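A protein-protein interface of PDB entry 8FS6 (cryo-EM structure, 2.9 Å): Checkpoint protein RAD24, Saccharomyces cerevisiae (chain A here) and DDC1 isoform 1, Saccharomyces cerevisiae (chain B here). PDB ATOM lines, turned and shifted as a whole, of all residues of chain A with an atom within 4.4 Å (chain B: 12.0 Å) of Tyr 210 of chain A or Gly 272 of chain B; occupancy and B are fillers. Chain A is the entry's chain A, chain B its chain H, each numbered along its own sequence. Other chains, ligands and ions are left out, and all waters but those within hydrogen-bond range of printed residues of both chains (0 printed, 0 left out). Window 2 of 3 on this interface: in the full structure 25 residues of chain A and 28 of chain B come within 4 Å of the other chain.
The side-chain hydroxyl of Tyr 210 of chain A sits at hydrogen-bond distance from the side-chain carboxylate of Glu 253 of chain A, at 2.8 Å.
Of the printed residues of chain B, Tyr 210 of chain A touches Val 270 (3.6 Å), Tyr 271 (3.2 Å), Gly 272 (3.8 Å), Lys 273 (3.4 Å) and Leu 278 (3.8 Å). Gly 272 of chain B touches just one residue of chain A: Tyr 210 (3.8 Å). No residue of chain B comes within 4 Å of Leu 206 of chain A. No residue of chain B comes within 4 Å of Leu 209 of chain A. Ser 212 of chain A touches three residues of chain B. Of the printed residues of chain A, Lys 268 of chain B touches Ser 212. Of the printed residues of chain B, Glu 253 of chain A touches Lys 273 (3.2 Å). His 257 of chain A touches none of the printed residues of chain B. The nearest residue of chain B that does not touch Tyr 210 of chain A is Ala 269 of chain B (6.3 Å).
Printed residues of chain B that touch a printed residue of chain A: Lys 268, Ala 269, Val 270, Tyr 271, Gly 272, Lys 273 and Leu 278. Hydrophobic or aromatic side chains of chain B that line the printed part of chain A: Val 270 and Leu 278. Among the printed residues, no Asp or Glu carboxylate lies within 4 Å of a Lys or Arg side-chain nitrogen of the other chain.
Gln 207 of chain A touches Leu 278 of chain B (NE2 to O, 3.7 Å). Val 270 of chain B touches Tyr 210 of chain A. CB of Tyr 210 of chain A touches O of Tyr 271 of chain B, at 3.2 Å. Tyr 210 of chain A touches Gly 272 of chain B (CD1 to O, 3.8 Å). OH of Tyr 210 of chain A touches CG of Lys 273 of chain B, at 3.4 Å. Tyr 210 of chain A touches Leu 278 of chain B (CD2 to CD1, 3.8 Å). Ser 211 of chain A touches Val 270 of chain B. Ala 269 of chain B touches Ser 212 of chain A (O to OG, 3.7 Å). Val 270 of chain B touches Ser 212 of chain A (CG1 to N, 3.9 Å). Glu 253 of chain A touches Lys 273 of chain B (OE2 to CG, 3.2 Å).
The side-chain hydroxyl (OG) of Ser 212 of chain A is in hydrogen-bond range of the side-chain amino group (NZ) of Lys 268 of chain B, 3.5 Å away.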
ATOM      1  N   LEU A 206      -1.437 -25.415  -6.855  1.00  0.00           N
ATOM      2  CA  LEU A 206      -1.364 -24.047  -7.361  1.00  0.00           C
ATOM      3  C   LEU A 206      -1.452 -24.015  -8.882  1.00  0.00           C
ATOM      4  O   LEU A 206      -2.088 -23.122  -9.455  1.00  0.00           O
ATOM      5  CB  LEU A 206      -0.074 -23.380  -6.885  1.00  0.00           C
ATOM      6  CG  LEU A 206      -0.230 -22.376  -5.742  1.00  0.00           C
ATOM      7  CD1 LEU A 206       1.052 -21.583  -5.540  1.00  0.00           C
ATOM      8  CD2 LEU A 206      -1.404 -21.451  -6.015  1.00  0.00           C
ATOM      9  N   GLN A 207      -0.809 -24.975  -9.550  1.00  0.00           N
ATOM     10  CA  GLN A 207      -0.917 -25.074 -11.002  1.00  0.00           C
ATOM     11  C   GLN A 207      -2.348 -25.357 -11.434  1.00  0.00           C
ATOM     12  O   GLN A 207      -2.813 -24.807 -12.438  1.00  0.00           O
ATOM     13  CB  GLN A 207       0.019 -26.164 -11.526  1.00  0.00           C
ATOM     14  CG  GLN A 207       1.491 -25.784 -11.519  1.00  0.00           C
ATOM     15  CD  GLN A 207       2.372 -26.866 -12.111  1.00  0.00           C
ATOM     16  OE1 GLN A 207       1.885 -27.805 -12.740  1.00  0.00           O
ATOM     17  NE2 GLN A 207       3.679 -26.742 -11.907  1.00  0.00           N
ATOM     18  N   TRP A 208      -3.052 -26.221 -10.698  1.00  0.00           N
ATOM     19  CA  TRP A 208      -4.463 -26.464 -10.990  1.00  0.00           C
ATOM     20  C   TRP A 208      -5.296 -25.204 -10.787  1.00  0.00           C
ATOM     21  O   TRP A 208      -6.171 -24.893 -11.604  1.00  0.00           O
ATOM     22  CB  TRP A 208      -4.991 -27.604 -10.117  1.00  0.00           C
ATOM     23  CG  TRP A 208      -6.409 -27.996 -10.422  1.00  0.00           C
ATOM     24  CD1 TRP A 208      -7.545 -27.391  -9.965  1.00  0.00           C
ATOM     25  CD2 TRP A 208      -6.841 -29.083 -11.250  1.00  0.00           C
ATOM     26  NE1 TRP A 208      -8.654 -28.033 -10.457  1.00  0.00           N
ATOM     27  CE2 TRP A 208      -8.250 -29.075 -11.250  1.00  0.00           C
ATOM     28  CE3 TRP A 208      -6.173 -30.061 -11.993  1.00  0.00           C
ATOM     29  CZ2 TRP A 208      -9.002 -30.007 -11.962  1.00  0.00           C
ATOM     30  CZ3 TRP A 208      -6.921 -30.985 -12.698  1.00  0.00           C
ATOM     31  CH2 TRP A 208      -8.321 -30.951 -12.678  1.00  0.00           C
ATOM     32  N   LEU A 209      -5.038 -24.465  -9.705  1.00  0.00           N
ATOM     33  CA  LEU A 209      -5.789 -23.246  -9.425  1.00  0.00           C
ATOM     34  C   LEU A 209      -5.462 -22.126 -10.402  1.00  0.00           C
ATOM     35  O   LEU A 209      -6.324 -21.280 -10.668  1.00  0.00           O
ATOM     36  CB  LEU A 209      -5.518 -22.778  -7.994  1.00  0.00           C
ATOM     37  CG  LEU A 209      -6.354 -23.428  -6.891  1.00  0.00           C
ATOM     38  CD1 LEU A 209      -5.745 -23.160  -5.524  1.00  0.00           C
ATOM     39  CD2 LEU A 209      -7.793 -22.939  -6.948  1.00  0.00           C
ATOM     40  N   TYR A 210      -4.242 -22.098 -10.937  1.00  0.00           N
ATOM     41  CA  TYR A 210      -3.829 -21.098 -11.914  1.00  0.00           C
ATOM     42  C   TYR A 210      -3.766 -21.668 -13.326  1.00  0.00           C
ATOM     43  O   TYR A 210      -3.056 -21.127 -14.179  1.00  0.00           O
ATOM     44  CB  TYR A 210      -2.476 -20.504 -11.524  1.00  0.00           C
ATOM     45  CG  TYR A 210      -2.557 -19.445 -10.449  1.00  0.00           C
ATOM     46  CD1 TYR A 210      -3.330 -18.304 -10.627  1.00  0.00           C
ATOM     47  CD2 TYR A 210      -1.858 -19.585  -9.259  1.00  0.00           C
ATOM     48  CE1 TYR A 210      -3.404 -17.333  -9.648  1.00  0.00           C
ATOM     49  CE2 TYR A 210      -1.926 -18.619  -8.275  1.00  0.00           C
ATOM     50  CZ  TYR A 210      -2.700 -17.496  -8.473  1.00  0.00           C
ATOM     51  OH  TYR A 210      -2.771 -16.533  -7.493  1.00  0.00           O
ATOM     52  N   SER A 211      -4.489 -22.756 -13.584  1.00  0.00           N
ATOM     53  CA  SER A 211      -4.441 -23.402 -14.888  1.00  0.00           C
ATOM     54  C   SER A 211      -5.077 -22.516 -15.951  1.00  0.00           C
ATOM     55  O   SER A 211      -6.147 -21.938 -15.737  1.00  0.00           O
ATOM     56  CB  SER A 211      -5.149 -24.754 -14.832  1.00  0.00           C
ATOM     57  OG  SER A 211      -5.487 -25.206 -16.131  1.00  0.00           O
ATOM     58  N   SER A 212      -4.413 -22.414 -17.102  1.00  0.00           N
ATOM     59  CA  SER A 212      -4.941 -21.652 -18.223  1.00  0.00           C
ATOM     60  C   SER A 212      -5.921 -22.451 -19.069  1.00  0.00           C
ATOM     61  O   SER A 212      -6.455 -21.911 -20.044  1.00  0.00           O
ATOM     62  CB  SER A 212      -3.796 -21.148 -19.105  1.00  0.00           C
ATOM     63  OG  SER A 212      -3.027 -22.226 -19.609  1.00  0.00           O
ATOM     64  N   GLU A 253      -1.320 -19.001   0.252  1.00  0.00           N
ATOM     65  CA  GLU A 253      -1.785 -18.589  -1.068  1.00  0.00           C
ATOM     66  C   GLU A 253      -2.928 -19.471  -1.561  1.00  0.00           C
ATOM     67  O   GLU A 253      -3.917 -18.967  -2.108  1.00  0.00           O
ATOM     68  CB  GLU A 253      -0.620 -18.605  -2.058  1.00  0.00           C
ATOM     69  CG  GLU A 253      -1.012 -18.877  -3.500  1.00  0.00           C
ATOM     70  CD  GLU A 253      -1.478 -17.636  -4.242  1.00  0.00           C
ATOM     71  OE1 GLU A 253      -2.160 -16.783  -3.639  1.00  0.00           O
ATOM     72  OE2 GLU A 253      -1.161 -17.519  -5.442  1.00  0.00           O
ATOM     73  N   HIS A 257      -6.768 -18.339  -2.004  1.00  0.00           N
ATOM     74  CA  HIS A 257      -6.969 -18.193  -3.437  1.00  0.00           C
ATOM     75  C   HIS A 257      -8.438 -17.895  -3.734  1.00  0.00           C
ATOM     76  O   HIS A 257      -9.329 -18.488  -3.116  1.00  0.00           O
ATOM     77  CB  HIS A 257      -6.532 -19.462  -4.168  1.00  0.00           C
ATOM     78  CG  HIS A 257      -6.280 -19.264  -5.631  1.00  0.00           C
ATOM     79  ND1 HIS A 257      -7.295 -19.232  -6.562  1.00  0.00           N
ATOM     80  CD2 HIS A 257      -5.129 -19.091  -6.322  1.00  0.00           C
ATOM     81  CE1 HIS A 257      -6.780 -19.045  -7.765  1.00  0.00           C
ATOM     82  NE2 HIS A 257      -5.468 -18.956  -7.646  1.00  0.00           N
ATOM     83  N   THR B 267       3.672 -28.577 -24.330  1.00  0.00           N
ATOM     84  CA  THR B 267       3.354 -28.452 -22.915  1.00  0.00           C
ATOM     85  C   THR B 267       2.794 -27.060 -22.666  1.00  0.00           C
ATOM     86  O   THR B 267       3.425 -26.064 -23.031  1.00  0.00           O
ATOM     87  CB  THR B 267       4.594 -28.696 -22.044  1.00  0.00           C
ATOM     88  OG1 THR B 267       4.835 -30.103 -21.941  1.00  0.00           O
ATOM     89  CG2 THR B 267       4.399 -28.121 -20.649  1.00  0.00           C
ATOM     90  N   LYS B 268       1.613 -26.996 -22.057  1.00  0.00           N
ATOM     91  CA  LYS B 268       1.001 -25.713 -21.752  1.00  0.00           C
ATOM     92  C   LYS B 268       1.736 -25.030 -20.601  1.00  0.00           C
ATOM     93  O   LYS B 268       2.330 -25.675 -19.732  1.00  0.00           O
ATOM     94  CB  LYS B 268      -0.476 -25.892 -21.402  1.00  0.00           C
ATOM     95  CG  LYS B 268      -1.322 -26.422 -22.548  1.00  0.00           C
ATOM     96  CD  LYS B 268      -2.798 -26.149 -22.314  1.00  0.00           C
ATOM     97  CE  LYS B 268      -3.071 -24.660 -22.188  1.00  0.00           C
ATOM     98  NZ  LYS B 268      -4.506 -24.379 -21.911  1.00  0.00           N
ATOM     99  N   ALA B 269       1.687 -23.699 -20.603  1.00  0.00           N
ATOM    100  CA  ALA B 269       2.352 -22.881 -19.593  1.00  0.00           C
ATOM    101  C   ALA B 269       1.292 -22.172 -18.762  1.00  0.00           C
ATOM    102  O   ALA B 269       0.580 -21.299 -19.269  1.00  0.00           O
ATOM    103  CB  ALA B 269       3.300 -21.873 -20.240  1.00  0.00           C
ATOM    104  N   VAL B 270       1.191 -22.544 -17.492  1.00  0.00           N
ATOM    105  CA  VAL B 270       0.300 -21.855 -16.568  1.00  0.00           C
ATOM    106  C   VAL B 270       1.029 -20.657 -15.973  1.00  0.00           C
ATOM    107  O   VAL B 270       2.256 -20.660 -15.818  1.00  0.00           O
ATOM    108  CB  VAL B 270      -0.210 -22.816 -15.475  1.00  0.00           C
ATOM    109  CG1 VAL B 270      -0.968 -23.974 -16.105  1.00  0.00           C
ATOM    110  CG2 VAL B 270       0.942 -23.331 -14.629  1.00  0.00           C
ATOM    111  N   TYR B 271       0.271 -19.615 -15.651  1.00  0.00           N
ATOM    112  CA  TYR B 271       0.824 -18.371 -15.140  1.00  0.00           C
ATOM    113  C   TYR B 271       0.401 -18.169 -13.692  1.00  0.00           C
ATOM    114  O   TYR B 271      -0.741 -18.457 -13.323  1.00  0.00           O
ATOM    115  CB  TYR B 271       0.376 -17.180 -15.991  1.00  0.00           C
ATOM    116  CG  TYR B 271       0.948 -17.187 -17.391  1.00  0.00           C
ATOM    117  CD1 TYR B 271       0.301 -17.855 -18.424  1.00  0.00           C
ATOM    118  CD2 TYR B 271       2.139 -16.534 -17.679  1.00  0.00           C
ATOM    119  CE1 TYR B 271       0.822 -17.867 -19.704  1.00  0.00           C
ATOM    120  CE2 TYR B 271       2.668 -16.541 -18.955  1.00  0.00           C
ATOM    121  CZ  TYR B 271       2.006 -17.208 -19.964  1.00  0.00           C
ATOM    122  OH  TYR B 271       2.529 -17.217 -21.237  1.00  0.00           O
ATOM    123  N   GLY B 272       1.327 -17.668 -12.878  1.00  0.00           N
ATOM    124  CA  GLY B 272       1.094 -17.492 -11.458  1.00  0.00           C
ATOM    125  C   GLY B 272       0.252 -16.277 -11.137  1.00  0.00           C
ATOM    126  O   GLY B 272      -0.654 -15.896 -11.889  1.00  0.00           O
ATOM    127  N   LYS B 273       0.546 -15.664  -9.989  1.00  0.00           N
ATOM    128  CA  LYS B 273      -0.211 -14.496  -9.548  1.00  0.00           C
ATOM    129  C   LYS B 273      -0.008 -13.318 -10.493  1.00  0.00           C
ATOM    130  O   LYS B 273      -0.970 -12.649 -10.888  1.00  0.00           O
ATOM    131  CB  LYS B 273       0.205 -14.114  -8.127  1.00  0.00           C
ATOM    132  CG  LYS B 273       0.348 -15.291  -7.182  1.00  0.00           C
ATOM    133  CD  LYS B 273       1.036 -14.883  -5.889  1.00  0.00           C
ATOM    134  CE  LYS B 273       0.295 -13.750  -5.197  1.00  0.00           C
ATOM    135  NZ  LYS B 273       0.979 -13.325  -3.944  1.00  0.00           N
ATOM    136  N   ASN B 274       1.239 -13.055 -10.869  1.00  0.00           N
ATOM    137  CA  ASN B 274       1.622 -11.884 -11.650  1.00  0.00           C
ATOM    138  C   ASN B 274       2.435 -12.298 -12.869  1.00  0.00           C
ATOM    139  O   ASN B 274       3.542 -11.805 -13.098  1.00  0.00           O
ATOM    140  CB  ASN B 274       2.402 -10.891 -10.794  1.00  0.00           C
ATOM    141  CG  ASN B 274       1.570 -10.310  -9.668  1.00  0.00           C
ATOM    142  OD1 ASN B 274       0.339 -10.335  -9.712  1.00  0.00           O
ATOM    143  ND2 ASN B 274       2.239  -9.781  -8.650  1.00  0.00           N
ATOM    144  N   ASN B 275       1.908 -13.257 -13.636  1.00  0.00           N
ATOM    145  CA  ASN B 275       2.457 -13.796 -14.886  1.00  0.00           C
ATOM    146  C   ASN B 275       3.621 -14.741 -14.565  1.00  0.00           C
ATOM    147  O   ASN B 275       4.171 -15.372 -15.479  1.00  0.00           O
ATOM    148  CB  ASN B 275       2.840 -12.664 -15.870  1.00  0.00           C
ATOM    149  CG  ASN B 275       3.743 -13.107 -17.011  1.00  0.00           C
ATOM    150  OD1 ASN B 275       4.965 -13.175 -16.866  1.00  0.00           O
ATOM    151  ND2 ASN B 275       3.141 -13.408 -18.156  1.00  0.00           N
ATOM    152  N   ASP B 276       3.942 -14.937 -13.283  1.00  0.00           N
ATOM    153  CA  ASP B 276       5.070 -15.766 -12.871  1.00  0.00           C
ATOM    154  C   ASP B 276       4.969 -17.174 -13.445  1.00  0.00           C
ATOM    155  O   ASP B 276       3.902 -17.793 -13.432  1.00  0.00           O
ATOM    156  CB  ASP B 276       5.135 -15.829 -11.343  1.00  0.00           C
ATOM    157  CG  ASP B 276       4.808 -14.501 -10.690  1.00  0.00           C
ATOM    158  OD1 ASP B 276       5.479 -13.498 -11.009  1.00  0.00           O
ATOM    159  OD2 ASP B 276       3.876 -14.460  -9.860  1.00  0.00           O
ATOM    160  N   LEU B 277       6.094 -17.672 -13.953  1.00  0.00           N
ATOM    161  CA  LEU B 277       6.149 -18.937 -14.685  1.00  0.00           C
ATOM    162  C   LEU B 277       6.085 -20.095 -13.696  1.00  0.00           C
ATOM    163  O   LEU B 277       7.105 -20.603 -13.228  1.00  0.00           O
ATOM    164  CB  LEU B 277       7.413 -19.005 -15.533  1.00  0.00           C
ATOM    165  CG  LEU B 277       7.470 -20.086 -16.613  1.00  0.00           C
ATOM    166  CD1 LEU B 277       6.337 -19.906 -17.610  1.00  0.00           C
ATOM    167  CD2 LEU B 277       8.818 -20.066 -17.318  1.00  0.00           C
ATOM    168  N   LEU B 278       4.861 -20.514 -13.366  1.00  0.00           N
ATOM    169  CA  LEU B 278       4.690 -21.711 -12.547  1.00  0.00           C
ATOM    170  C   LEU B 278       5.138 -22.956 -13.304  1.00  0.00           C
ATOM    171  O   LEU B 278       5.833 -23.815 -12.751  1.00  0.00           O
ATOM    172  CB  LEU B 278       3.232 -21.843 -12.106  1.00  0.00           C
ATOM    173  CG  LEU B 278       2.752 -20.898 -11.003  1.00  0.00           C
ATOM    174  CD1 LEU B 278       1.264 -21.091 -10.749  1.00  0.00           C
ATOM    175  CD2 LEU B 278       3.550 -21.108  -9.725  1.00  0.00           C
ATOM    176  N   ARG B 279       4.747 -23.067 -14.572  1.00  0.00           N
ATOM    177  CA  ARG B 279       5.149 -24.172 -15.432  1.00  0.00           C
ATOM    178  C   ARG B 279       5.553 -23.614 -16.788  1.00  0.00           C
ATOM    179  O   ARG B 279       4.812 -22.825 -17.383  1.00  0.00           O
ATOM    180  CB  ARG B 279       4.016 -25.194 -15.590  1.00  0.00           C
ATOM    181  CG  ARG B 279       4.354 -26.370 -16.491  1.00  0.00           C
ATOM    182  CD  ARG B 279       3.198 -27.355 -16.566  1.00  0.00           C
ATOM    183  NE  ARG B 279       3.523 -28.521 -17.379  1.00  0.00           N
ATOM    184  CZ  ARG B 279       4.076 -29.632 -16.911  1.00  0.00           C
ATOM    185  NH1 ARG B 279       4.380 -29.766 -15.630  1.00  0.00           N
ATOM    186  NH2 ARG B 279       4.329 -30.634 -17.748  1.00  0.00           N
ATOM    187  N   ASN B 280       6.722 -24.024 -17.272  1.00  0.00           N
ATOM    188  CA  ASN B 280       7.227 -23.543 -18.548  1.00  0.00           C
ATOM    189  C   ASN B 280       6.626 -24.344 -19.703  1.00  0.00           C
ATOM    190  O   ASN B 280       6.053 -25.422 -19.521  1.00  0.00           O
ATOM    191  CB  ASN B 280       8.753 -23.611 -18.577  1.00  0.00           C
ATOM    192  CG  ASN B 280       9.285 -24.952 -18.113  1.00  0.00           C
ATOM    193  OD1 ASN B 280       8.539 -25.783 -17.594  1.00  0.00           O
ATOM    194  ND2 ASN B 280      10.582 -25.169 -18.294  1.00  0.00           N
ATOM    195  N   ALA B 281       6.765 -23.799 -20.909  1.00  0.00           N
ATOM    196  CA  ALA B 281       6.201 -24.391 -22.116  1.00  0.00           C
ATOM    197  C   ALA B 281       7.327 -24.881 -23.015  1.00  0.00           C
ATOM    198  O   ALA B 281       8.185 -24.092 -23.428  1.00  0.00           O
ATOM    199  CB  ALA B 281       5.325 -23.383 -22.861  1.00  0.00           C
